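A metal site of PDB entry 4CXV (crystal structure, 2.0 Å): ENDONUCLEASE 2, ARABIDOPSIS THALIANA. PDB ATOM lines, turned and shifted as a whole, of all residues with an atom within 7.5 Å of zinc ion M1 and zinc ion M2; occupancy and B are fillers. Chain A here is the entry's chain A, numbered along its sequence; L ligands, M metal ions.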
ATOM      1  N   TRP A   1       3.148  12.048   6.972  1.00  0.00           N
ATOM      2  CA  TRP A   1       2.879  10.608   7.116  1.00  0.00           C
ATOM      3  C   TRP A   1       4.147   9.812   7.282  1.00  0.00           C
ATOM      4  O   TRP A   1       5.203  10.213   6.825  1.00  0.00           O
ATOM      5  CB  TRP A   1       2.146  10.016   5.894  1.00  0.00           C
ATOM      6  CG  TRP A   1       0.997  10.816   5.434  1.00  0.00           C
ATOM      7  CD1 TRP A   1       0.986  11.684   4.402  1.00  0.00           C
ATOM      8  CD2 TRP A   1      -0.348  10.779   5.951  1.00  0.00           C
ATOM      9  NE1 TRP A   1      -0.278  12.225   4.257  1.00  0.00           N
ATOM     10  CE2 TRP A   1      -1.103  11.689   5.209  1.00  0.00           C
ATOM     11  CE3 TRP A   1      -0.962  10.060   6.989  1.00  0.00           C
ATOM     12  CZ2 TRP A   1      -2.453  11.924   5.474  1.00  0.00           C
ATOM     13  CZ3 TRP A   1      -2.298  10.293   7.239  1.00  0.00           C
ATOM     14  CH2 TRP A   1      -3.028  11.229   6.490  1.00  0.00           C
ATOM     15  N   GLY A   2       3.999   8.652   7.895  1.00  0.00           N
ATOM     16  CA  GLY A   2       5.050   7.624   7.858  1.00  0.00           C
ATOM     17  C   GLY A   2       5.057   6.880   6.532  1.00  0.00           C
ATOM     18  O   GLY A   2       4.430   7.260   5.557  1.00  0.00           O
ATOM     19  N   LYS A   3       5.773   5.778   6.530  1.00  0.00           N
ATOM     20  CA  LYS A   3       6.050   5.043   5.301  1.00  0.00           C
ATOM     21  C   LYS A   3       4.797   4.620   4.585  1.00  0.00           C
ATOM     22  O   LYS A   3       4.674   4.768   3.370  1.00  0.00           O
ATOM     23  CB  LYS A   3       6.831   3.766   5.665  1.00  0.00           C
ATOM     24  CG  LYS A   3       7.367   2.995   4.459  1.00  0.00           C
ATOM     25  CD  LYS A   3       6.374   2.004   3.903  1.00  0.00           C
ATOM     26  CE  LYS A   3       6.976   0.606   3.782  1.00  0.00           C
ATOM     27  NZ  LYS A   3       8.295   0.598   3.134  1.00  0.00           N
ATOM     28  N   GLY A   5       1.632   5.684   4.702  1.00  0.00           N
ATOM     29  CA  GLY A   5       0.826   6.752   4.109  1.00  0.00           C
ATOM     30  C   GLY A   5       1.411   7.249   2.797  1.00  0.00           C
ATOM     31  O   GLY A   5       0.702   7.427   1.833  1.00  0.00           O
ATOM     32  N   HIS A   6       2.718   7.514   2.785  1.00  0.00           N
ATOM     33  CA  HIS A   6       3.354   7.976   1.545  1.00  0.00           C
ATOM     34  C   HIS A   6       3.283   6.915   0.439  1.00  0.00           C
ATOM     35  O   HIS A   6       3.085   7.251  -0.727  1.00  0.00           O
ATOM     36  CB  HIS A   6       4.808   8.435   1.800  1.00  0.00           C
ATOM     37  CG  HIS A   6       4.915   9.731   2.544  1.00  0.00           C
ATOM     38  ND1 HIS A   6       4.662  10.939   1.950  1.00  0.00           N
ATOM     39  CD2 HIS A   6       5.227   9.999   3.831  1.00  0.00           C
ATOM     40  CE1 HIS A   6       4.846  11.908   2.828  1.00  0.00           C
ATOM     41  NE2 HIS A   6       5.141  11.359   3.986  1.00  0.00           N
ATOM     42  N   CYS A  41       9.037   7.470  -2.209  1.00  0.00           N
ATOM     43  CA  CYS A  41       8.225   8.561  -1.633  1.00  0.00           C
ATOM     44  C   CYS A  41       8.516   8.861  -0.174  1.00  0.00           C
ATOM     45  O   CYS A  41       7.938   9.782   0.382  1.00  0.00           O
ATOM     46  CB  CYS A  41       6.745   8.386  -1.908  1.00  0.00           C
ATOM     47  SG  CYS A  41       6.404   8.670  -3.662  1.00  0.00           S
ATOM     48  N   LEU A  42       9.474   8.151   0.422  1.00  0.00           N
ATOM     49  CA  LEU A  42      10.018   8.520   1.736  1.00  0.00           C
ATOM     50  C   LEU A  42      11.431   9.135   1.654  1.00  0.00           C
ATOM     51  O   LEU A  42      11.990   9.506   2.669  1.00  0.00           O
ATOM     52  CB  LEU A  42      10.006   7.322   2.690  1.00  0.00           C
ATOM     53  CG  LEU A  42       9.567   7.564   4.129  1.00  0.00           C
ATOM     54  CD1 LEU A  42       8.102   8.024   4.226  1.00  0.00           C
ATOM     55  CD2 LEU A  42       9.760   6.280   4.891  1.00  0.00           C
ATOM     56  N   ALA A  44      12.480  12.009   0.894  1.00  0.00           N
ATOM     57  CA  ALA A  44      12.625  13.315   1.517  1.00  0.00           C
ATOM     58  C   ALA A  44      12.830  13.210   3.019  1.00  0.00           C
ATOM     59  O   ALA A  44      13.501  14.045   3.594  1.00  0.00           O
ATOM     60  CB  ALA A  44      11.448  14.230   1.207  1.00  0.00           C
ATOM     61  N   ASP A  45      12.183  12.254   3.667  1.00  0.00           N
ATOM     62  CA  ASP A  45      12.348  12.159   5.128  1.00  0.00           C
ATOM     63  C   ASP A  45      13.811  11.829   5.518  1.00  0.00           C
ATOM     64  O   ASP A  45      14.266  12.244   6.565  1.00  0.00           O
ATOM     65  CB  ASP A  45      11.406  11.111   5.742  1.00  0.00           C
ATOM     66  CG  ASP A  45      10.030  11.700   6.131  1.00  0.00           C
ATOM     67  OD1 ASP A  45       9.783  12.917   5.967  1.00  0.00           O
ATOM     68  OD2 ASP A  45       9.195  10.912   6.591  1.00  0.00           O
ATOM     69  N   LYS A  48      16.308  15.031   5.842  1.00  0.00           N
ATOM     70  CA  LYS A  48      16.037  16.082   6.821  1.00  0.00           C
ATOM     71  C   LYS A  48      17.285  16.701   7.455  1.00  0.00           C
ATOM     72  O   LYS A  48      17.221  17.853   7.870  1.00  0.00           O
ATOM     73  CB  LYS A  48      15.087  15.569   7.901  1.00  0.00           C
ATOM     74  CG  LYS A  48      13.663  15.416   7.435  1.00  0.00           C
ATOM     75  CD  LYS A  48      12.735  15.115   8.613  1.00  0.00           C
ATOM     76  CE  LYS A  48      11.326  14.906   8.158  1.00  0.00           C
ATOM     77  NZ  LYS A  48      10.481  14.271   9.222  1.00  0.00           N
ATOM     78  N   SER A  55      14.143  20.466   6.377  1.00  0.00           N
ATOM     79  CA  SER A  55      13.271  19.932   7.439  1.00  0.00           C
ATOM     80  C   SER A  55      12.001  20.754   7.678  1.00  0.00           C
ATOM     81  O   SER A  55      10.945  20.177   7.939  1.00  0.00           O
ATOM     82  CB  SER A  55      13.924  19.537   8.783  1.00  0.00           C
ATOM     83  OG  SER A  55      15.079  20.254   9.108  1.00  0.00           O
ATOM     84  N   LEU A  57      10.318  22.158   5.499  1.00  0.00           N
ATOM     85  CA  LEU A  57       9.481  22.034   4.319  1.00  0.00           C
ATOM     86  C   LEU A  57       8.447  20.921   4.426  1.00  0.00           C
ATOM     87  O   LEU A  57       7.635  20.782   3.516  1.00  0.00           O
ATOM     88  CB  LEU A  57      10.367  21.793   3.082  1.00  0.00           C
ATOM     89  CG  LEU A  57      11.478  22.825   2.824  1.00  0.00           C
ATOM     90  CD1 LEU A  57      12.189  22.538   1.507  1.00  0.00           C
ATOM     91  CD2 LEU A  57      10.938  24.256   2.829  1.00  0.00           C
ATOM     92  N   HIS A  58       8.475  20.137   5.503  1.00  0.00           N
ATOM     93  CA  HIS A  58       7.539  19.025   5.650  1.00  0.00           C
ATOM     94  C   HIS A  58       6.211  19.432   6.291  1.00  0.00           C
ATOM     95  O   HIS A  58       5.267  18.628   6.276  1.00  0.00           O
ATOM     96  CB  HIS A  58       8.190  17.886   6.458  1.00  0.00           C
ATOM     97  CG  HIS A  58       9.359  17.249   5.758  1.00  0.00           C
ATOM     98  ND1 HIS A  58       9.322  15.953   5.297  1.00  0.00           N
ATOM     99  CD2 HIS A  58      10.582  17.717   5.427  1.00  0.00           C
ATOM    100  CE1 HIS A  58      10.477  15.647   4.723  1.00  0.00           C
ATOM    101  NE2 HIS A  58      11.259  16.702   4.788  1.00  0.00           N
ATOM    102  N   TYR A  59       6.098  20.632   6.832  1.00  0.00           N
ATOM    103  CA  TYR A  59       4.921  20.974   7.619  1.00  0.00           C
ATOM    104  C   TYR A  59       4.669  22.487   7.584  1.00  0.00           C
ATOM    105  O   TYR A  59       5.400  23.247   6.939  1.00  0.00           O
ATOM    106  CB  TYR A  59       5.121  20.498   9.069  1.00  0.00           C
ATOM    107  CG  TYR A  59       6.362  21.081   9.702  1.00  0.00           C
ATOM    108  CD1 TYR A  59       6.347  22.367  10.227  1.00  0.00           C
ATOM    109  CD2 TYR A  59       7.588  20.390   9.679  1.00  0.00           C
ATOM    110  CE1 TYR A  59       7.485  22.936  10.774  1.00  0.00           C
ATOM    111  CE2 TYR A  59       8.727  20.933  10.247  1.00  0.00           C
ATOM    112  CZ  TYR A  59       8.662  22.203  10.795  1.00  0.00           C
ATOM    113  OH  TYR A  59       9.762  22.770  11.320  1.00  0.00           O
ATOM    114  N   VAL A  85       5.638  23.499   3.918  1.00  0.00           N
ATOM    115  CA  VAL A  85       5.276  22.513   2.909  1.00  0.00           C
ATOM    116  C   VAL A  85       4.540  23.109   1.702  1.00  0.00           C
ATOM    117  O   VAL A  85       4.717  22.643   0.581  1.00  0.00           O
ATOM    118  CB  VAL A  85       4.591  21.285   3.540  1.00  0.00           C
ATOM    119  CG1 VAL A  85       3.202  21.639   4.086  1.00  0.00           C
ATOM    120  CG2 VAL A  85       4.531  20.120   2.564  1.00  0.00           C
ATOM    121  N   HIS A 120       6.572  13.543  -2.014  1.00  0.00           N
ATOM    122  CA  HIS A 120       6.495  13.433  -0.578  1.00  0.00           C
ATOM    123  C   HIS A 120       5.701  14.594   0.046  1.00  0.00           C
ATOM    124  O   HIS A 120       4.857  14.375   0.908  1.00  0.00           O
ATOM    125  CB  HIS A 120       7.902  13.389   0.004  1.00  0.00           C
ATOM    126  CG  HIS A 120       7.916  13.254   1.492  1.00  0.00           C
ATOM    127  ND1 HIS A 120       7.940  12.031   2.117  1.00  0.00           N
ATOM    128  CD2 HIS A 120       7.930  14.171   2.466  1.00  0.00           C
ATOM    129  CE1 HIS A 120       7.985  12.213   3.422  1.00  0.00           C
ATOM    130  NE2 HIS A 120       7.946  13.504   3.667  1.00  0.00           N
ATOM    131  N   PHE A 121       6.001  15.816  -0.384  1.00  0.00           N
ATOM    132  CA  PHE A 121       5.364  16.987   0.210  1.00  0.00           C
ATOM    133  C   PHE A 121       3.872  17.075  -0.138  1.00  0.00           C
ATOM    134  O   PHE A 121       3.087  17.514   0.695  1.00  0.00           O
ATOM    135  CB  PHE A 121       6.139  18.268  -0.113  1.00  0.00           C
ATOM    136  CG  PHE A 121       7.562  18.313   0.455  1.00  0.00           C
ATOM    137  CD1 PHE A 121       7.879  17.775   1.690  1.00  0.00           C
ATOM    138  CD2 PHE A 121       8.578  18.937  -0.266  1.00  0.00           C
ATOM    139  CE1 PHE A 121       9.152  17.870   2.214  1.00  0.00           C
ATOM    140  CE2 PHE A 121       9.864  19.016   0.246  1.00  0.00           C
ATOM    141  CZ  PHE A 121      10.156  18.465   1.487  1.00  0.00           C
ATOM    142  N   GLY A 123       2.053  14.553  -0.235  1.00  0.00           N
ATOM    143  CA  GLY A 123       1.548  13.712   0.834  1.00  0.00           C
ATOM    144  C   GLY A 123       1.487  14.410   2.170  1.00  0.00           C
ATOM    145  O   GLY A 123       0.436  14.436   2.826  1.00  0.00           O
ATOM    146  N   ASP A 124       2.598  15.007   2.601  1.00  0.00           N
ATOM    147  CA  ASP A 124       2.643  15.612   3.917  1.00  0.00           C
ATOM    148  C   ASP A 124       1.615  16.734   4.074  1.00  0.00           C
ATOM    149  O   ASP A 124       1.069  16.882   5.155  1.00  0.00           O
ATOM    150  CB  ASP A 124       4.001  16.144   4.264  1.00  0.00           C
ATOM    151  CG  ASP A 124       4.872  15.121   4.886  1.00  0.00           C
ATOM    152  OD1 ASP A 124       4.455  13.950   5.076  1.00  0.00           O
ATOM    153  OD2 ASP A 124       5.986  15.475   5.163  1.00  0.00           O
ATOM    154  N   ILE A 125       1.363  17.533   3.042  1.00  0.00           N
ATOM    155  CA  ILE A 125       0.403  18.634   3.172  1.00  0.00           C
ATOM    156  C   ILE A 125      -1.017  18.127   3.413  1.00  0.00           C
ATOM    157  O   ILE A 125      -1.860  18.908   3.858  1.00  0.00           O
ATOM    158  CB  ILE A 125       0.492  19.625   1.976  1.00  0.00           C
ATOM    159  CG1 ILE A 125      -0.085  20.981   2.369  1.00  0.00           C
ATOM    160  CG2 ILE A 125      -0.162  19.109   0.706  1.00  0.00           C
ATOM    161  CD1 ILE A 125       0.280  22.118   1.436  1.00  0.00           C
ATOM    162  N   GLN A 127      -1.551  15.450   5.574  1.00  0.00           N
ATOM    163  CA  GLN A 127      -1.605  14.899   6.926  1.00  0.00           C
ATOM    164  C   GLN A 127      -2.094  16.084   7.822  1.00  0.00           C
ATOM    165  O   GLN A 127      -1.440  17.123   7.890  1.00  0.00           O
ATOM    166  CB  GLN A 127      -0.208  14.437   7.375  1.00  0.00           C
ATOM    167  CG  GLN A 127      -0.192  13.286   8.376  1.00  0.00           C
ATOM    168  CD  GLN A 127      -0.525  13.692   9.793  1.00  0.00           C
ATOM    169  OE1 GLN A 127      -1.607  14.254  10.067  1.00  0.00           O
ATOM    170  NE2 GLN A 127       0.350  13.346  10.724  1.00  0.00           N
ATOM    171  N   HIS A 130       0.292  17.935   9.995  1.00  0.00           N
ATOM    172  CA  HIS A 130       1.352  18.702   9.348  1.00  0.00           C
ATOM    173  C   HIS A 130       0.930  20.141   9.029  1.00  0.00           C
ATOM    174  O   HIS A 130       1.722  20.867   8.466  1.00  0.00           O
ATOM    175  CB  HIS A 130       1.851  17.960   8.086  1.00  0.00           C
ATOM    176  CG  HIS A 130       2.833  16.881   8.388  1.00  0.00           C
ATOM    177  ND1 HIS A 130       4.133  16.907   7.928  1.00  0.00           N
ATOM    178  CD2 HIS A 130       2.727  15.751   9.137  1.00  0.00           C
ATOM    179  CE1 HIS A 130       4.783  15.846   8.364  1.00  0.00           C
ATOM    180  NE2 HIS A 130       3.952  15.115   9.089  1.00  0.00           N
ATOM    181  N   HIS A 154       0.769  13.263  17.041  1.00  0.00           N
ATOM    182  CA  HIS A 154       1.309  13.402  15.706  1.00  0.00           C
ATOM    183  C   HIS A 154       1.616  12.046  15.072  1.00  0.00           C
ATOM    184  O   HIS A 154       1.245  11.771  13.927  1.00  0.00           O
ATOM    185  CB  HIS A 154       2.542  14.244  15.716  1.00  0.00           C
ATOM    186  CG  HIS A 154       3.009  14.597  14.355  1.00  0.00           C
ATOM    187  ND1 HIS A 154       2.646  15.761  13.717  1.00  0.00           N
ATOM    188  CD2 HIS A 154       3.740  13.880  13.461  1.00  0.00           C
ATOM    189  CE1 HIS A 154       3.185  15.776  12.516  1.00  0.00           C
ATOM    190  NE2 HIS A 154       3.848  14.645  12.338  1.00  0.00           N
ATOM    191  N   ASP A 158       0.482  10.166  11.704  1.00  0.00           N
ATOM    192  CA  ASP A 158       1.434   9.751  10.678  1.00  0.00           C
ATOM    193  C   ASP A 158       1.332   8.257  10.373  1.00  0.00           C
ATOM    194  O   ASP A 158       1.370   7.873   9.185  1.00  0.00           O
ATOM    195  CB  ASP A 158       2.872  10.020  11.108  1.00  0.00           C
ATOM    196  CG  ASP A 158       3.343  11.396  10.764  1.00  0.00           C
ATOM    197  OD1 ASP A 158       2.704  12.116   9.972  1.00  0.00           O
ATOM    198  OD2 ASP A 158       4.409  11.781  11.301  1.00  0.00           O
HETATM  199  P1  LIG L   1       7.062  13.032   7.917  1.00  0.00           P
HETATM  200  O1  LIG L   1       7.943  11.869   8.360  1.00  0.00           O
HETATM  201  O2  LIG L   1       6.539  12.809   6.527  1.00  0.00           O
HETATM  202  O3  LIG L   1       7.783  14.330   7.708  1.00  0.00           O
HETATM  203  O4  LIG L   1       5.939  12.954   8.889  1.00  0.00           O
HETATM  204 ZN    ZN M   1       5.033  12.133   5.818  1.00  0.00          ZN
HETATM  205 ZN    ZN M   2       7.783  14.341   5.630  1.00  0.00          ZN
HETATM  206 ZN    ZN M   3       4.740  13.685  10.482  1.00  0.00          ZN
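O of His 58 sits at hydrogen-bond distance from ND1 of His 130 (2.6 Å).
ND1 of His 120 lies close to ND1 of His 6, at 3.5 Å.
The backbone carbonyl oxygen (O) of Gly 123 sits at hydrogen-bond distance from the indole nitrogen (NE1) of Trp 1, 2.7 Å away.
A ring nitrogen (ND1) of His 120 is in hydrogen-bond range of the backbone carbonyl oxygen (O) of Cys 41, 2.8 Å away.
The side-chain carboxylate (OD1) of Asp 45 sits close to the side-chain amino group (NZ) of Lys 48 (3.6 Å).
The backbone NH (N) of Trp 1 lies close to the side-chain carboxylate (OD1) of Asp 158 (3.0 Å).
The nearest printed residue that does not touch zinc ion M1 is Gly 2 (4.2 Å).
Of the 24 residues printed, 4 come within 4 Å of zinc ion M2.
The nearest printed residue that does not touch zinc ion M2 is His 6 (4.3 Å).
Zinc ion M1 is bound by an oxygen (O2) of the ligand (1.8 Å), a ring nitrogen (NE2) of His 6 (2.0 Å), the side-chain carboxylate (OD1) of Asp 124 (2.0 Å), the backbone carbonyl oxygen (O) of Trp 1 (2.2 Å) and the backbone nitrogen (N) of Trp 1 (2.2 Å).
O3 of the ligand binds zinc ion M2 (2.1 Å).
Zinc ion M2 is bound by NE2 of His 120.
An oxygen (O2) of the ligand is bound to zinc ion M2 (2.2 Å).
OD2 of Asp 124 is bound to zinc ion M2, at 2.2 Å.
Zinc ion M2 is bound by a ring nitrogen (ND1) of His 58, at 2.3 Å.
The side-chain carboxylate (OD1) of Asp 45 is bound to zinc ion M2 (2.5 Å).
Zinc ion M2 has six donor atoms within binding distance.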
